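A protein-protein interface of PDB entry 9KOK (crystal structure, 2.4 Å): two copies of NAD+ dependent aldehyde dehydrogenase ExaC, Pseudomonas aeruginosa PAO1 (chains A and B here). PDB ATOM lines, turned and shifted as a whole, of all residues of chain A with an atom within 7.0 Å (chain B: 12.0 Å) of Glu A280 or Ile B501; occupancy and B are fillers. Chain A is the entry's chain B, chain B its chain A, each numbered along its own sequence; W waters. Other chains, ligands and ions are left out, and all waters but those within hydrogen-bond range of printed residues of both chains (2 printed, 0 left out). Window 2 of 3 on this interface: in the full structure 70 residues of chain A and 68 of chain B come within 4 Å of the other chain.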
ATOM      1  N   ASP A 275      -6.732  35.927  -0.052  1.00  0.00           N
ATOM      2  CA  ASP A 275      -6.232  34.649   0.451  1.00  0.00           C
ATOM      3  C   ASP A 275      -6.711  33.456  -0.371  1.00  0.00           C
ATOM      4  O   ASP A 275      -6.132  32.372  -0.252  1.00  0.00           O
ATOM      5  CB  ASP A 275      -6.602  34.443   1.924  1.00  0.00           C
ATOM      6  CG  ASP A 275      -8.104  34.253   2.141  1.00  0.00           C
ATOM      7  OD1 ASP A 275      -8.853  35.244   2.054  1.00  0.00           O
ATOM      8  OD2 ASP A 275      -8.543  33.106   2.396  1.00  0.00           O
ATOM      9  N   ILE A 276      -7.725  33.617  -1.220  1.00  0.00           N
ATOM     10  CA  ILE A 276      -8.160  32.457  -1.993  1.00  0.00           C
ATOM     11  C   ILE A 276      -7.076  31.989  -2.967  1.00  0.00           C
ATOM     12  O   ILE A 276      -7.071  30.821  -3.364  1.00  0.00           O
ATOM     13  CB  ILE A 276      -9.495  32.731  -2.734  1.00  0.00           C
ATOM     14  CG1 ILE A 276      -9.271  33.632  -3.951  1.00  0.00           C
ATOM     15  CG2 ILE A 276     -10.561  33.342  -1.770  1.00  0.00           C
ATOM     16  CD1 ILE A 276     -10.543  34.030  -4.679  1.00  0.00           C
ATOM     17  N   MET A 277      -6.167  32.873  -3.393  1.00  0.00           N
ATOM     18  CA  MET A 277      -5.073  32.404  -4.244  1.00  0.00           C
ATOM     19  C   MET A 277      -3.964  31.693  -3.486  1.00  0.00           C
ATOM     20  O   MET A 277      -3.055  31.141  -4.125  1.00  0.00           O
ATOM     21  CB  MET A 277      -4.506  33.511  -5.130  1.00  0.00           C
ATOM     22  CG  MET A 277      -5.535  34.473  -5.605  1.00  0.00           C
ATOM     23  SD  MET A 277      -6.387  33.643  -6.971  1.00  0.00           S
ATOM     24  CE  MET A 277      -5.040  32.964  -7.936  1.00  0.00           C
ATOM     25  N   GLN A 278      -4.032  31.665  -2.161  1.00  0.00           N
ATOM     26  CA  GLN A 278      -3.187  30.796  -1.364  1.00  0.00           C
ATOM     27  C   GLN A 278      -3.824  29.428  -1.134  1.00  0.00           C
ATOM     28  O   GLN A 278      -3.250  28.613  -0.419  1.00  0.00           O
ATOM     29  CB  GLN A 278      -2.913  31.440  -0.002  1.00  0.00           C
ATOM     30  CG  GLN A 278      -1.515  31.903   0.223  1.00  0.00           C
ATOM     31  CD  GLN A 278      -1.228  33.146  -0.561  1.00  0.00           C
ATOM     32  OE1 GLN A 278      -1.726  34.226  -0.229  1.00  0.00           O
ATOM     33  NE2 GLN A 278      -0.436  33.010  -1.625  1.00  0.00           N
ATOM     34  N   ALA A 279      -5.004  29.164  -1.695  1.00  0.00           N
ATOM     35  CA  ALA A 279      -5.730  27.937  -1.393  1.00  0.00           C
ATOM     36  C   ALA A 279      -5.377  26.831  -2.388  1.00  0.00           C
ATOM     37  O   ALA A 279      -4.448  26.951  -3.188  1.00  0.00           O
ATOM     38  CB  ALA A 279      -7.231  28.215  -1.356  1.00  0.00           C
ATOM     39  N   GLU A 280      -6.123  25.733  -2.349  1.00  0.00           N
ATOM     40  CA  GLU A 280      -5.877  24.638  -3.265  1.00  0.00           C
ATOM     41  C   GLU A 280      -6.212  25.064  -4.695  1.00  0.00           C
ATOM     42  O   GLU A 280      -7.055  25.946  -4.908  1.00  0.00           O
ATOM     43  CB  GLU A 280      -6.708  23.426  -2.873  1.00  0.00           C
ATOM     44  CG  GLU A 280      -6.588  23.037  -1.394  1.00  0.00           C
ATOM     45  CD  GLU A 280      -7.534  23.827  -0.471  1.00  0.00           C
ATOM     46  OE1 GLU A 280      -8.144  24.803  -0.913  1.00  0.00           O
ATOM     47  OE2 GLU A 280      -7.670  23.479   0.707  1.00  0.00           O
ATOM     48  N   PRO A 281      -5.555  24.461  -5.698  1.00  0.00           N
ATOM     49  CA  PRO A 281      -5.903  24.791  -7.092  1.00  0.00           C
ATOM     50  C   PRO A 281      -7.366  24.538  -7.422  1.00  0.00           C
ATOM     51  O   PRO A 281      -7.987  25.349  -8.128  1.00  0.00           O
ATOM     52  CB  PRO A 281      -4.968  23.887  -7.910  1.00  0.00           C
ATOM     53  CG  PRO A 281      -3.817  23.616  -6.991  1.00  0.00           C
ATOM     54  CD  PRO A 281      -4.399  23.552  -5.610  1.00  0.00           C
ATOM     55  N   ALA A 282      -7.933  23.435  -6.927  1.00  0.00           N
ATOM     56  CA  ALA A 282      -9.356  23.186  -7.135  1.00  0.00           C
ATOM     57  C   ALA A 282     -10.197  24.328  -6.573  1.00  0.00           C
ATOM     58  O   ALA A 282     -11.153  24.780  -7.220  1.00  0.00           O
ATOM     59  CB  ALA A 282      -9.756  21.856  -6.508  1.00  0.00           C
ATOM     60  N   PHE A 283      -9.808  24.858  -5.410  1.00  0.00           N
ATOM     61  CA  PHE A 283     -10.577  25.930  -4.793  1.00  0.00           C
ATOM     62  C   PHE A 283     -10.540  27.204  -5.625  1.00  0.00           C
ATOM     63  O   PHE A 283     -11.547  27.921  -5.715  1.00  0.00           O
ATOM     64  CB  PHE A 283     -10.057  26.225  -3.396  1.00  0.00           C
ATOM     65  CG  PHE A 283     -10.876  27.244  -2.675  1.00  0.00           C
ATOM     66  CD1 PHE A 283     -12.085  26.892  -2.104  1.00  0.00           C
ATOM     67  CD2 PHE A 283     -10.474  28.565  -2.621  1.00  0.00           C
ATOM     68  CE1 PHE A 283     -12.856  27.827  -1.443  1.00  0.00           C
ATOM     69  CE2 PHE A 283     -11.238  29.508  -1.960  1.00  0.00           C
ATOM     70  CZ  PHE A 283     -12.439  29.136  -1.371  1.00  0.00           C
ATOM     71  N   ILE A 284      -9.384  27.518  -6.214  1.00  0.00           N
ATOM     72  CA  ILE A 284      -9.289  28.689  -7.082  1.00  0.00           C
ATOM     73  C   ILE A 284     -10.187  28.519  -8.294  1.00  0.00           C
ATOM     74  O   ILE A 284     -10.852  29.461  -8.735  1.00  0.00           O
ATOM     75  CB  ILE A 284      -7.831  28.943  -7.491  1.00  0.00           C
ATOM     76  CG1 ILE A 284      -7.027  29.466  -6.297  1.00  0.00           C
ATOM     77  CG2 ILE A 284      -7.779  29.912  -8.676  1.00  0.00           C
ATOM     78  CD1 ILE A 284      -5.517  29.266  -6.439  1.00  0.00           C
ATOM     79  N   GLU A 285     -10.213  27.311  -8.851  1.00  0.00           N
ATOM     80  CA  GLU A 285     -11.115  27.013  -9.953  1.00  0.00           C
ATOM     81  C   GLU A 285     -12.568  27.218  -9.537  1.00  0.00           C
ATOM     82  O   GLU A 285     -13.352  27.835 -10.271  1.00  0.00           O
ATOM     83  CB  GLU A 285     -10.881  25.577 -10.416  1.00  0.00           C
ATOM     84  CG  GLU A 285     -10.895  25.402 -11.908  1.00  0.00           C
ATOM     85  CD  GLU A 285     -11.165  23.967 -12.313  1.00  0.00           C
ATOM     86  OE1 GLU A 285     -10.356  23.086 -11.922  1.00  0.00           O
ATOM     87  OE2 GLU A 285     -12.182  23.734 -13.018  1.00  0.00           O
ATOM     88  N   LYS A 286     -12.936  26.716  -8.344  1.00  0.00           N
ATOM     89  CA  LYS A 286     -14.305  26.850  -7.852  1.00  0.00           C
ATOM     90  C   LYS A 286     -14.692  28.313  -7.720  1.00  0.00           C
ATOM     91  O   LYS A 286     -15.798  28.701  -8.101  1.00  0.00           O
ATOM     92  CB  LYS A 286     -14.466  26.143  -6.501  1.00  0.00           C
ATOM     93  CG  LYS A 286     -15.721  26.569  -5.742  1.00  0.00           C
ATOM     94  CD  LYS A 286     -15.929  25.851  -4.392  1.00  0.00           C
ATOM     95  CE  LYS A 286     -17.379  25.377  -4.277  1.00  0.00           C
ATOM     96  NZ  LYS A 286     -17.865  25.265  -2.876  1.00  0.00           N
ATOM     97  N   ALA A 287     -13.790  29.136  -7.173  1.00  0.00           N
ATOM     98  CA  ALA A 287     -14.069  30.559  -7.056  1.00  0.00           C
ATOM     99  C   ALA A 287     -14.225  31.188  -8.430  1.00  0.00           C
ATOM    100  O   ALA A 287     -15.083  32.057  -8.632  1.00  0.00           O
ATOM    101  CB  ALA A 287     -12.949  31.252  -6.279  1.00  0.00           C
ATOM    102  N   ARG A 438     -11.028  32.072   2.988  1.00  0.00           N
ATOM    103  CA  ARG A 438     -10.831  30.879   3.796  1.00  0.00           C
ATOM    104  C   ARG A 438     -10.459  31.198   5.241  1.00  0.00           C
ATOM    105  O   ARG A 438     -10.259  30.272   6.035  1.00  0.00           O
ATOM    106  CB  ARG A 438      -9.785  29.977   3.132  1.00  0.00           C
ATOM    107  CG  ARG A 438     -10.338  29.283   1.888  1.00  0.00           C
ATOM    108  CD  ARG A 438     -11.307  28.141   2.276  1.00  0.00           C
ATOM    109  NE  ARG A 438     -10.553  26.996   2.779  1.00  0.00           N
ATOM    110  CZ  ARG A 438      -9.883  26.152   2.001  1.00  0.00           C
ATOM    111  NH1 ARG A 438     -10.001  26.183   0.677  1.00  0.00           N
ATOM    112  NH2 ARG A 438      -9.029  25.297   2.558  1.00  0.00           N
ATOM    113  N   ASN A 458     -18.141  30.854  -0.085  1.00  0.00           N
ATOM    114  CA  ASN A 458     -17.313  29.889  -0.824  1.00  0.00           C
ATOM    115  C   ASN A 458     -18.167  28.956  -1.693  1.00  0.00           C
ATOM    116  O   ASN A 458     -17.865  27.771  -1.864  1.00  0.00           O
ATOM    117  CB  ASN A 458     -16.400  29.129   0.147  1.00  0.00           C
ATOM    118  CG  ASN A 458     -15.410  30.091   0.840  1.00  0.00           C
ATOM    119  OD1 ASN A 458     -15.021  31.104   0.244  1.00  0.00           O
ATOM    120  ND2 ASN A 458     -15.038  29.807   2.090  1.00  0.00           N
ATOM    121  N   ASN B 144     -26.162  19.113   3.038  1.00  0.00           N
ATOM    122  CA  ASN B 144     -25.505  17.858   2.733  1.00  0.00           C
ATOM    123  C   ASN B 144     -24.167  17.876   3.440  1.00  0.00           C
ATOM    124  O   ASN B 144     -23.875  18.780   4.234  1.00  0.00           O
ATOM    125  CB  ASN B 144     -25.376  17.618   1.224  1.00  0.00           C
ATOM    126  CG  ASN B 144     -24.607  18.718   0.493  1.00  0.00           C
ATOM    127  OD1 ASN B 144     -23.657  19.308   1.009  1.00  0.00           O
ATOM    128  ND2 ASN B 144     -25.019  18.983  -0.724  1.00  0.00           N
ATOM    129  N   ASP B 145     -23.358  16.859   3.162  1.00  0.00           N
ATOM    130  CA  ASP B 145     -22.123  16.670   3.912  1.00  0.00           C
ATOM    131  C   ASP B 145     -21.204  17.903   3.871  1.00  0.00           C
ATOM    132  O   ASP B 145     -20.411  18.121   4.793  1.00  0.00           O
ATOM    133  CB  ASP B 145     -21.416  15.434   3.367  1.00  0.00           C
ATOM    134  CG  ASP B 145     -20.185  15.103   4.138  1.00  0.00           C
ATOM    135  OD1 ASP B 145     -20.276  14.966   5.384  1.00  0.00           O
ATOM    136  OD2 ASP B 145     -19.124  15.018   3.492  1.00  0.00           O
ATOM    137  N   SER B 146     -21.284  18.730   2.830  1.00  0.00           N
ATOM    138  CA  SER B 146     -20.376  19.870   2.745  1.00  0.00           C
ATOM    139  C   SER B 146     -21.116  21.197   2.591  1.00  0.00           C
ATOM    140  O   SER B 146     -20.512  22.193   2.173  1.00  0.00           O
ATOM    141  CB  SER B 146     -19.381  19.670   1.600  1.00  0.00           C
ATOM    142  OG  SER B 146     -20.065  19.623   0.369  1.00  0.00           O
ATOM    143  N   THR B 147     -22.411  21.241   2.918  1.00  0.00           N
ATOM    144  CA  THR B 147     -23.184  22.476   2.805  1.00  0.00           C
ATOM    145  C   THR B 147     -24.033  22.675   4.051  1.00  0.00           C
ATOM    146  O   THR B 147     -24.887  21.845   4.371  1.00  0.00           O
ATOM    147  CB  THR B 147     -24.080  22.461   1.568  1.00  0.00           C
ATOM    148  OG1 THR B 147     -23.353  21.916   0.469  1.00  0.00           O
ATOM    149  CG2 THR B 147     -24.564  23.900   1.241  1.00  0.00           C
ATOM    150  N   VAL B 148     -23.848  23.792   4.725  1.00  0.00           N
ATOM    151  CA  VAL B 148     -24.600  24.048   5.938  1.00  0.00           C
ATOM    152  C   VAL B 148     -25.301  25.390   5.794  1.00  0.00           C
ATOM    153  O   VAL B 148     -24.689  26.375   5.375  1.00  0.00           O
ATOM    154  CB  VAL B 148     -23.697  24.020   7.186  1.00  0.00           C
ATOM    155  CG1 VAL B 148     -24.497  24.432   8.427  1.00  0.00           C
ATOM    156  CG2 VAL B 148     -23.085  22.601   7.369  1.00  0.00           C
ATOM    157  N   VAL B 497     -23.060  28.083   3.633  1.00  0.00           N
ATOM    158  CA  VAL B 497     -21.614  27.838   3.593  1.00  0.00           C
ATOM    159  C   VAL B 497     -21.330  26.486   2.960  1.00  0.00           C
ATOM    160  O   VAL B 497     -21.902  25.461   3.373  1.00  0.00           O
ATOM    161  CB  VAL B 497     -20.988  27.910   4.990  1.00  0.00           C
ATOM    162  CG1 VAL B 497     -19.459  27.814   4.883  1.00  0.00           C
ATOM    163  CG2 VAL B 497     -21.421  29.201   5.680  1.00  0.00           C
ATOM    164  N   SER B 498     -20.460  26.492   1.944  1.00  0.00           N
ATOM    165  CA  SER B 498     -19.924  25.276   1.346  1.00  0.00           C
ATOM    166  C   SER B 498     -18.510  25.021   1.864  1.00  0.00           C
ATOM    167  O   SER B 498     -17.667  25.924   1.873  1.00  0.00           O
ATOM    168  CB  SER B 498     -19.894  25.379  -0.176  1.00  0.00           C
ATOM    169  OG  SER B 498     -19.370  24.183  -0.706  1.00  0.00           O
ATOM    170  N   TYR B 499     -18.262  23.795   2.309  1.00  0.00           N
ATOM    171  CA  TYR B 499     -16.943  23.372   2.761  1.00  0.00           C
ATOM    172  C   TYR B 499     -16.275  22.454   1.748  1.00  0.00           C
ATOM    173  O   TYR B 499     -15.271  21.823   2.063  1.00  0.00           O
ATOM    174  CB  TYR B 499     -17.044  22.690   4.125  1.00  0.00           C
ATOM    175  CG  TYR B 499     -17.747  23.543   5.146  1.00  0.00           C
ATOM    176  CD1 TYR B 499     -17.098  24.619   5.738  1.00  0.00           C
ATOM    177  CD2 TYR B 499     -19.068  23.298   5.495  1.00  0.00           C
ATOM    178  CE1 TYR B 499     -17.728  25.401   6.651  1.00  0.00           C
ATOM    179  CE2 TYR B 499     -19.718  24.083   6.427  1.00  0.00           C
ATOM    180  CZ  TYR B 499     -19.049  25.133   7.004  1.00  0.00           C
ATOM    181  OH  TYR B 499     -19.686  25.931   7.936  1.00  0.00           O
ATOM    182  N   ASP B 500     -16.846  22.337   0.560  1.00  0.00           N
ATOM    183  CA  ASP B 500     -16.270  21.599  -0.550  1.00  0.00           C
ATOM    184  C   ASP B 500     -15.407  22.558  -1.371  1.00  0.00           C
ATOM    185  O   ASP B 500     -15.844  23.669  -1.680  1.00  0.00           O
ATOM    186  CB  ASP B 500     -17.418  21.038  -1.397  1.00  0.00           C
ATOM    187  CG  ASP B 500     -16.977  20.045  -2.464  1.00  0.00           C
ATOM    188  OD1 ASP B 500     -15.796  20.026  -2.870  1.00  0.00           O
ATOM    189  OD2 ASP B 500     -17.865  19.326  -2.973  1.00  0.00           O
ATOM    190  N   ILE B 501     -14.190  22.129  -1.731  1.00  0.00           N
ATOM    191  CA  ILE B 501     -13.309  22.971  -2.532  1.00  0.00           C
ATOM    192  C   ILE B 501     -13.487  22.762  -4.033  1.00  0.00           C
ATOM    193  O   ILE B 501     -12.906  23.519  -4.822  1.00  0.00           O
ATOM    194  CB  ILE B 501     -11.819  22.770  -2.162  1.00  0.00           C
ATOM    195  CG1 ILE B 501     -11.317  21.371  -2.499  1.00  0.00           C
ATOM    196  CG2 ILE B 501     -11.585  23.070  -0.697  1.00  0.00           C
ATOM    197  CD1 ILE B 501      -9.790  21.273  -2.440  1.00  0.00           C
ATOM    198  N   ASN B 502     -14.371  21.805  -4.467  1.00  0.00           N
ATOM    199  CA  ASN B 502     -14.363  21.533  -5.898  1.00  0.00           C
ATOM    200  C   ASN B 502     -15.434  22.325  -6.627  1.00  0.00           C
ATOM    201  O   ASN B 502     -16.478  22.653  -6.055  1.00  0.00           O
ATOM    202  CB  ASN B 502     -14.588  20.050  -6.170  1.00  0.00           C
ATOM    203  CG  ASN B 502     -13.530  19.205  -5.539  1.00  0.00           C
ATOM    204  OD1 ASN B 502     -13.796  18.469  -4.591  1.00  0.00           O
ATOM    205  ND2 ASN B 502     -12.297  19.354  -6.013  1.00  0.00           N
ATOM    206  N   PRO B 503     -15.167  22.634  -7.893  1.00  0.00           N
ATOM    207  CA  PRO B 503     -16.185  23.263  -8.737  1.00  0.00           C
ATOM    208  C   PRO B 503     -17.428  22.393  -8.885  1.00  0.00           C
ATOM    209  O   PRO B 503     -17.405  21.170  -8.719  1.00  0.00           O
ATOM    210  CB  PRO B 503     -15.472  23.438 -10.089  1.00  0.00           C
ATOM    211  CG  PRO B 503     -13.991  23.332  -9.784  1.00  0.00           C
ATOM    212  CD  PRO B 503     -13.879  22.444  -8.589  1.00  0.00           C
ATOM    213  N   LEU B 504     -18.536  23.052  -9.235  1.00  0.00           N
ATOM    214  CA  LEU B 504     -19.801  22.347  -9.380  1.00  0.00           C
ATOM    215  C   LEU B 504     -19.864  21.538 -10.674  1.00  0.00           C
ATOM    216  O   LEU B 504     -20.620  20.565 -10.752  1.00  0.00           O
ATOM    217  CB  LEU B 504     -20.968  23.340  -9.315  1.00  0.00           C
ATOM    218  CG  LEU B 504     -21.263  24.069  -8.001  1.00  0.00           C
ATOM    219  CD1 LEU B 504     -22.479  24.951  -8.168  1.00  0.00           C
ATOM    220  CD2 LEU B 504     -21.496  23.083  -6.856  1.00  0.00           C
ATOM    221  N   GLY B 505     -19.119  21.936 -11.703  1.00  0.00           N
ATOM    222  CA  GLY B 505     -19.235  21.328 -13.013  1.00  0.00           C
ATOM    223  C   GLY B 505     -20.085  22.089 -14.014  1.00  0.00           C
ATOM    224  O   GLY B 505     -20.380  21.547 -15.083  1.00  0.00           O
ATOM    225  N   PHE B 506     -20.485  23.325 -13.715  1.00  0.00           N
ATOM    226  CA  PHE B 506     -21.279  24.076 -14.682  1.00  0.00           C
ATOM    227  C   PHE B 506     -20.455  25.041 -15.507  1.00  0.00           C
ATOM    228  O   PHE B 506     -20.721  25.197 -16.699  1.00  0.00           O
ATOM    229  CB  PHE B 506     -22.399  24.851 -13.984  1.00  0.00           C
ATOM    230  CG  PHE B 506     -23.532  23.996 -13.603  1.00  0.00           C
ATOM    231  CD1 PHE B 506     -24.500  23.656 -14.536  1.00  0.00           C
ATOM    232  CD2 PHE B 506     -23.606  23.471 -12.328  1.00  0.00           C
ATOM    233  CE1 PHE B 506     -25.557  22.822 -14.198  1.00  0.00           C
ATOM    234  CE2 PHE B 506     -24.650  22.643 -11.981  1.00  0.00           C
ATOM    235  CZ  PHE B 506     -25.633  22.320 -12.918  1.00  0.00           C
ATOM    236  N   PHE B 507     -19.458  25.686 -14.919  1.00  0.00           N
ATOM    237  CA  PHE B 507     -18.653  26.626 -15.690  1.00  0.00           C
ATOM    238  C   PHE B 507     -17.190  26.461 -15.330  1.00  0.00           C
ATOM    239  O   PHE B 507     -16.320  26.980 -16.041  1.00  0.00           O
ATOM    240  CB  PHE B 507     -19.105  28.071 -15.465  1.00  0.00           C
ATOM    241  CG  PHE B 507     -20.463  28.388 -16.046  1.00  0.00           C
ATOM    242  CD1 PHE B 507     -20.613  28.635 -17.412  1.00  0.00           C
ATOM    243  CD2 PHE B 507     -21.586  28.457 -15.228  1.00  0.00           C
ATOM    244  CE1 PHE B 507     -21.866  28.950 -17.961  1.00  0.00           C
ATOM    245  CE2 PHE B 507     -22.855  28.768 -15.763  1.00  0.00           C
ATOM    246  CZ  PHE B 507     -22.990  29.014 -17.141  1.00  0.00           C
ATOM    247  OXT PHE B 507     -16.853  25.804 -14.333  1.00  0.00           O
HETATM  248  O   HOH W   1     -20.388  23.616  -3.590  1.00  0.00           O
HETATM  249  O   HOH W   2     -16.100  27.380   3.430  1.00  0.00           O
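N of Asp B500 is in hydrogen-bond range of OG of Ser B498 (3.4 Å). The side-chain carboxylate of Asp B500 is in hydrogen-bond range of the backbone NH of Asn B502, 2.8 Å away. The side-chain carboxylate of Asp A275 is in hydrogen-bond range of the backbone NH of Arg A438. OE1 of Glu A280 lies within salt-bridge range of NH1 of Arg A438 (2.8 Å). The side-chain amino group of Lys A286 lies within hydrogen-bond range of the backbone carbonyl oxygen of Asn A458, at 2.7 Å.
CB of Glu A280 touches CD1 of Ile B501, at 3.8 Å. Ala A282 touches Asn B502. Pro B503 touches Ala A282 (CD to O, 3.8 Å). Pro B503 touches Glu A285 (CG to OE2, 3.7 Å). CB of Lys A286 touches O of Ile B501, 3.5 Å away. Lys A286 touches Asn B502. Lys A286 touches Pro B503. CG2 of Ile B501 touches NH1 of Arg A438, at 3.8 Å. O of Asn A458 touches CB of Ser B498, 3.6 Å away.
OG of Ser B498 sits at hydrogen-bond distance from NZ of Lys A286, at 2.9 Å. The backbone carbonyl oxygen of Asp B500 sits at hydrogen-bond distance from the side-chain amino group of Lys A286, at 2.8 Å. The backbone carbonyl oxygen (O) of Ile B501 lies close to the backbone NH (N) of Phe A283. O of Ala A282 sits close to O of Ile B501 (3.2 Å).
Of the 15 printed residues of chain A, 7 touch a printed residue of chain B. Printed residues of chain A that touch a printed residue of chain B: Glu A280, Ala A282, Phe A283, Glu A285, Lys A286, Arg A438 and Asn A458. Hydrophobic or aromatic side chains of chain A within 4 Å of the printed part of chain B: Ala A282. Printed residues of chain B that touch a printed residue of chain A: Ser B498, Asp B500, Ile B501, Asn B502 and Pro B503. Hydrophobic or aromatic side chains of chain B that line the printed part of chain A: Ile B501 and Pro B503. Among the printed residues, 13 pairs touch across the chains. Among the printed residues, no Asp or Glu carboxylate lies within 4 Å of a Lys or Arg side-chain nitrogen of the other chain.
No position is printed for both chains.
Glu A280 touches just one residue of chain B: Ile B501 (3.8 Å). No residue of chain B comes within 4 Å of Ala A279. No residue of chain B comes within 4 Å of Pro A281. Of chain B, only Ile B501, Asn B502 and Pro B503 come within 4 Å of Ala A282. No residue of chain B comes within 4 Å of Ile A284. Printed residues of chain B within 4 Å of Glu A285: Pro B503. Printed residues of chain B within 4 Å of Arg A438: Ile B501. Of the printed residues of chain A, Asp B500 touches Lys A286. Of the printed residues of chain A, Ser B498 touches Lys A286 and Asn A458. Printed residues of chain B within 4 Å of Asn A458: Ser B498 (3.6 Å). The nearest residue of chain A that does not touch Ile B501 is Ile A284 (5.5 Å).
Water W2 lies within hydrogen-bond range of O of Ser B498 (2.6 Å) and ND2 of Asn A458 (3.0 Å). Water W1 lies within hydrogen-bond range of NZ of Lys A286 (3.1 Å) and OG of Ser B498 (3.1 Å).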
